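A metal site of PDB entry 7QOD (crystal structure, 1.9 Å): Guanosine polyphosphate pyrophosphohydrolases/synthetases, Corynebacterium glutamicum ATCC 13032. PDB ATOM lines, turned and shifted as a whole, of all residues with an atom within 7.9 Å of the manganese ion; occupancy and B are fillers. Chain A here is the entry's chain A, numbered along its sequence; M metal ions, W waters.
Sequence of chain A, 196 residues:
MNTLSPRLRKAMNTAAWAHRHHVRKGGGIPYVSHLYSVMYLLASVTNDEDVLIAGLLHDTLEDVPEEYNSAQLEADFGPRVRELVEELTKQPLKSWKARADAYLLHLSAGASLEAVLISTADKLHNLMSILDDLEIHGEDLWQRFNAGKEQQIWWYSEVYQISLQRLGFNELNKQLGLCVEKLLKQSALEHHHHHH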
ATOM      1  N   TYR A  31     -11.579 -31.825  20.677  1.00  0.00           N
ATOM      2  CA  TYR A  31     -10.672 -31.220  21.667  1.00  0.00           C
ATOM      3  C   TYR A  31     -11.078 -29.803  22.079  1.00  0.00           C
ATOM      4  O   TYR A  31     -10.703 -29.352  23.178  1.00  0.00           O
ATOM      5  CB  TYR A  31      -9.265 -31.160  21.098  1.00  0.00           C
ATOM      6  CG  TYR A  31      -8.199 -31.045  22.153  1.00  0.00           C
ATOM      7  CD1 TYR A  31      -7.824 -32.158  22.883  1.00  0.00           C
ATOM      8  CD2 TYR A  31      -7.570 -29.818  22.434  1.00  0.00           C
ATOM      9  CE1 TYR A  31      -6.868 -32.093  23.869  1.00  0.00           C
ATOM     10  CE2 TYR A  31      -6.592 -29.751  23.411  1.00  0.00           C
ATOM     11  CZ  TYR A  31      -6.246 -30.886  24.132  1.00  0.00           C
ATOM     12  OH  TYR A  31      -5.257 -30.844  25.122  1.00  0.00           O
ATOM     13  N   HIS A  34     -12.365 -29.015  25.555  1.00  0.00           N
ATOM     14  CA  HIS A  34     -11.395 -28.731  26.616  1.00  0.00           C
ATOM     15  C   HIS A  34     -10.958 -27.266  26.570  1.00  0.00           C
ATOM     16  O   HIS A  34     -10.870 -26.599  27.612  1.00  0.00           O
ATOM     17  CB  HIS A  34     -10.173 -29.659  26.459  1.00  0.00           C
ATOM     18  CG  HIS A  34      -8.943 -29.219  27.209  1.00  0.00           C
ATOM     19  ND1 HIS A  34      -8.843 -29.246  28.587  1.00  0.00           N
ATOM     20  CD2 HIS A  34      -7.720 -28.836  26.746  1.00  0.00           C
ATOM     21  CE1 HIS A  34      -7.627 -28.841  28.947  1.00  0.00           C
ATOM     22  NE2 HIS A  34      -6.917 -28.611  27.848  1.00  0.00           N
ATOM     23  N   LEU A  35     -10.725 -26.737  25.367  1.00  0.00           N
ATOM     24  CA  LEU A  35     -10.214 -25.376  25.235  1.00  0.00           C
ATOM     25  C   LEU A  35     -11.220 -24.349  25.721  1.00  0.00           C
ATOM     26  O   LEU A  35     -10.866 -23.399  26.448  1.00  0.00           O
ATOM     27  CB  LEU A  35      -9.825 -25.108  23.777  1.00  0.00           C
ATOM     28  CG  LEU A  35      -8.789 -26.097  23.248  1.00  0.00           C
ATOM     29  CD1 LEU A  35      -8.497 -25.801  21.793  1.00  0.00           C
ATOM     30  CD2 LEU A  35      -7.497 -26.030  24.085  1.00  0.00           C
ATOM     31  N   VAL A  38     -11.548 -24.491  29.474  1.00  0.00           N
ATOM     32  CA  VAL A  38     -10.438 -23.777  30.106  1.00  0.00           C
ATOM     33  C   VAL A  38     -10.652 -22.266  30.071  1.00  0.00           C
ATOM     34  O   VAL A  38     -10.405 -21.559  31.064  1.00  0.00           O
ATOM     35  CB  VAL A  38      -9.112 -24.193  29.430  1.00  0.00           C
ATOM     36  CG1 VAL A  38      -8.024 -23.203  29.817  1.00  0.00           C
ATOM     37  CG2 VAL A  38      -8.718 -25.589  29.912  1.00  0.00           C
ATOM     38  N   GLY A  55      -5.653 -18.990  26.999  1.00  0.00           N
ATOM     39  CA  GLY A  55      -6.339 -20.206  27.440  1.00  0.00           C
ATOM     40  C   GLY A  55      -6.996 -20.950  26.284  1.00  0.00           C
ATOM     41  O   GLY A  55      -6.921 -22.179  26.200  1.00  0.00           O
ATOM     42  N   HIS A  58      -3.953 -22.515  24.175  1.00  0.00           N
ATOM     43  CA  HIS A  58      -2.756 -22.964  24.888  1.00  0.00           C
ATOM     44  C   HIS A  58      -2.211 -24.294  24.391  1.00  0.00           C
ATOM     45  O   HIS A  58      -1.042 -24.585  24.631  1.00  0.00           O
ATOM     46  CB  HIS A  58      -3.036 -23.052  26.410  1.00  0.00           C
ATOM     47  CG  HIS A  58      -3.861 -24.250  26.803  1.00  0.00           C
ATOM     48  ND1 HIS A  58      -5.237 -24.241  26.800  1.00  0.00           N
ATOM     49  CD2 HIS A  58      -3.493 -25.461  27.292  1.00  0.00           C
ATOM     50  CE1 HIS A  58      -5.687 -25.415  27.204  1.00  0.00           C
ATOM     51  NE2 HIS A  58      -4.651 -26.162  27.543  1.00  0.00           N
ATOM     52  N   ASP A  59      -3.014 -25.114  23.712  1.00  0.00           N
ATOM     53  CA  ASP A  59      -2.502 -26.369  23.185  1.00  0.00           C
ATOM     54  C   ASP A  59      -2.225 -26.343  21.680  1.00  0.00           C
ATOM     55  O   ASP A  59      -1.828 -27.369  21.142  1.00  0.00           O
ATOM     56  CB  ASP A  59      -3.482 -27.513  23.495  1.00  0.00           C
ATOM     57  CG  ASP A  59      -3.364 -27.974  24.944  1.00  0.00           C
ATOM     58  OD1 ASP A  59      -2.277 -27.799  25.509  1.00  0.00           O
ATOM     59  OD2 ASP A  59      -4.359 -28.470  25.500  1.00  0.00           O
ATOM     60  N   THR A  60      -2.421 -25.198  21.004  1.00  0.00           N
ATOM     61  CA  THR A  60      -2.214 -25.150  19.544  1.00  0.00           C
ATOM     62  C   THR A  60      -0.799 -25.550  19.162  1.00  0.00           C
ATOM     63  O   THR A  60      -0.601 -26.391  18.281  1.00  0.00           O
ATOM     64  CB  THR A  60      -2.493 -23.755  18.976  1.00  0.00           C
ATOM     65  OG1 THR A  60      -1.747 -22.767  19.703  1.00  0.00           O
ATOM     66  CG2 THR A  60      -3.993 -23.421  19.021  1.00  0.00           C
ATOM     67  N   ASP A  63      -0.069 -29.352  20.072  1.00  0.00           N
ATOM     68  CA  ASP A  63      -0.879 -30.435  19.535  1.00  0.00           C
ATOM     69  C   ASP A  63      -1.223 -30.310  18.056  1.00  0.00           C
ATOM     70  O   ASP A  63      -1.360 -31.332  17.366  1.00  0.00           O
ATOM     71  CB  ASP A  63      -2.187 -30.556  20.316  1.00  0.00           C
ATOM     72  CG  ASP A  63      -1.949 -30.957  21.763  1.00  0.00           C
ATOM     73  OD1 ASP A  63      -0.894 -31.536  22.023  1.00  0.00           O
ATOM     74  OD2 ASP A  63      -2.800 -30.689  22.627  1.00  0.00           O
ATOM     75  N   LEU A  88       4.218 -22.414  28.421  1.00  0.00           N
ATOM     76  CA  LEU A  88       3.820 -23.763  28.798  1.00  0.00           C
ATOM     77  C   LEU A  88       4.520 -24.872  27.998  1.00  0.00           C
ATOM     78  O   LEU A  88       4.178 -26.037  28.183  1.00  0.00           O
ATOM     79  CB  LEU A  88       2.306 -23.919  28.658  1.00  0.00           C
ATOM     80  CG  LEU A  88       1.489 -22.792  29.280  1.00  0.00           C
ATOM     81  CD1 LEU A  88       0.001 -23.012  29.029  1.00  0.00           C
ATOM     82  CD2 LEU A  88       1.779 -22.723  30.754  1.00  0.00           C
ATOM     83  N   ILE A 118      -3.227 -19.973  33.797  1.00  0.00           N
ATOM     84  CA  ILE A 118      -3.680 -20.744  32.642  1.00  0.00           C
ATOM     85  C   ILE A 118      -3.406 -22.226  32.868  1.00  0.00           C
ATOM     86  O   ILE A 118      -4.251 -23.096  32.587  1.00  0.00           O
ATOM     87  CB  ILE A 118      -2.979 -20.248  31.360  1.00  0.00           C
ATOM     88  CG1 ILE A 118      -3.397 -18.827  31.035  1.00  0.00           C
ATOM     89  CG2 ILE A 118      -3.236 -21.205  30.214  1.00  0.00           C
ATOM     90  CD1 ILE A 118      -2.462 -18.116  30.009  1.00  0.00           C
ATOM     91  N   SER A 119      -2.221 -22.530  33.362  1.00  0.00           N
ATOM     92  CA  SER A 119      -1.859 -23.913  33.640  1.00  0.00           C
ATOM     93  C   SER A 119      -2.776 -24.519  34.685  1.00  0.00           C
ATOM     94  O   SER A 119      -3.151 -25.689  34.587  1.00  0.00           O
ATOM     95  CB  SER A 119      -0.403 -23.952  34.082  1.00  0.00           C
ATOM     96  OG  SER A 119      -0.017 -25.242  34.502  1.00  0.00           O
ATOM     97  N   ALA A 121      -5.993 -23.656  35.197  1.00  0.00           N
ATOM     98  CA  ALA A 121      -7.279 -23.943  34.558  1.00  0.00           C
ATOM     99  C   ALA A 121      -7.190 -25.194  33.681  1.00  0.00           C
ATOM    100  O   ALA A 121      -8.118 -26.006  33.642  1.00  0.00           O
ATOM    101  CB  ALA A 121      -7.750 -22.736  33.732  1.00  0.00           C
ATOM    102  N   ASP A 122      -6.084 -25.333  32.954  1.00  0.00           N
ATOM    103  CA  ASP A 122      -5.831 -26.514  32.135  1.00  0.00           C
ATOM    104  C   ASP A 122      -5.827 -27.782  32.971  1.00  0.00           C
ATOM    105  O   ASP A 122      -6.485 -28.765  32.639  1.00  0.00           O
ATOM    106  CB  ASP A 122      -4.493 -26.301  31.425  1.00  0.00           C
ATOM    107  CG  ASP A 122      -4.037 -27.489  30.595  1.00  0.00           C
ATOM    108  OD1 ASP A 122      -4.857 -28.176  29.981  1.00  0.00           O
ATOM    109  OD2 ASP A 122      -2.805 -27.686  30.524  1.00  0.00           O
ATOM    110  N   LYS A 123      -5.032 -27.807  34.032  1.00  0.00           N
ATOM    111  CA  LYS A 123      -4.926 -29.008  34.863  1.00  0.00           C
ATOM    112  C   LYS A 123      -6.237 -29.284  35.592  1.00  0.00           C
ATOM    113  O   LYS A 123      -6.637 -30.441  35.734  1.00  0.00           O
ATOM    114  CB  LYS A 123      -3.784 -28.820  35.871  1.00  0.00           C
ATOM    115  CG  LYS A 123      -2.646 -29.752  35.551  1.00  0.00           C
ATOM    116  CD  LYS A 123      -2.109 -29.506  34.141  1.00  0.00           C
ATOM    117  CE  LYS A 123      -1.299 -28.241  34.123  1.00  0.00           C
ATOM    118  NZ  LYS A 123      -0.848 -27.884  32.727  1.00  0.00           N
ATOM    119  N   HIS A 125      -9.354 -28.577  34.454  1.00  0.00           N
ATOM    120  CA  HIS A 125     -10.325 -29.209  33.575  1.00  0.00           C
ATOM    121  C   HIS A 125      -9.893 -30.630  33.225  1.00  0.00           C
ATOM    122  O   HIS A 125     -10.744 -31.518  33.066  1.00  0.00           O
ATOM    123  CB  HIS A 125     -10.559 -28.405  32.282  1.00  0.00           C
ATOM    124  CG  HIS A 125     -11.555 -29.053  31.374  1.00  0.00           C
ATOM    125  ND1 HIS A 125     -11.202 -29.744  30.239  1.00  0.00           N
ATOM    126  CD2 HIS A 125     -12.897 -29.205  31.512  1.00  0.00           C
ATOM    127  CE1 HIS A 125     -12.288 -30.243  29.683  1.00  0.00           C
ATOM    128  NE2 HIS A 125     -13.328 -29.933  30.434  1.00  0.00           N
ATOM    129  N   ASN A 126      -8.592 -30.883  33.093  1.00  0.00           N
ATOM    130  CA  ASN A 126      -8.140 -32.240  32.807  1.00  0.00           C
ATOM    131  C   ASN A 126      -8.479 -33.187  33.964  1.00  0.00           C
ATOM    132  O   ASN A 126      -8.893 -34.319  33.750  1.00  0.00           O
ATOM    133  CB  ASN A 126      -6.645 -32.251  32.522  1.00  0.00           C
ATOM    134  CG  ASN A 126      -6.320 -31.692  31.128  1.00  0.00           C
ATOM    135  OD1 ASN A 126      -7.172 -31.690  30.259  1.00  0.00           O
ATOM    136  ND2 ASN A 126      -5.128 -31.194  30.932  1.00  0.00           N
HETATM  137 MN    MN M   1      -4.672 -28.386  27.826  1.00  0.00          MN
HETATM  138  O   HOH W   1      -2.601 -28.486  27.966  1.00  0.00           O
HETATM  139  O   HOH W   2      -4.583 -30.552  27.944  1.00  0.00           O
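A ring nitrogen (ND1) of His 34 sits close to the side-chain amide oxygen (OD1) of Asn 126, at 3.4 Å. O of Gly 55 lies within hydrogen-bond range of ND1 of His 58, 2.7 Å away. OD2 of Asp 59 lies close to OH of Tyr 31, 2.6 Å away. A ring nitrogen (ND1) of His 125 is in hydrogen-bond range of a ring nitrogen (ND1) of His 34 (2.9 Å). ND2 of Asn 126 sits at hydrogen-bond distance from O of Asp 122 (3.3 Å). The side-chain carboxylate of Asp 122 is in salt-bridge range of the side-chain amino group of Lys 123.
Merely in contact with the manganese ion: Tyr 31. Within 4 Å of the manganese ion: Tyr 31, His 34, His 58, Asp 59 and Asp 122. The nearest printed residue that does not touch the manganese ion is Asn 126 (4.2 Å).
The manganese ion is bound by water W1, water W2, the side-chain carboxylate (OD1) of Asp 122, a ring nitrogen (NE2) of His 58, a ring nitrogen (NE2) of His 34 and the side-chain carboxylate (OD2) of Asp 59.
Water W1 bridges OD1 of Asp 59 (2.6 Å) and OD2 of Asp 122 (2.7 Å). Water W2 bridges the side-chain hydroxyl of Tyr 31 (2.9 Å) and the side-chain amide nitrogen of Asn 126 (3.1 Å).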
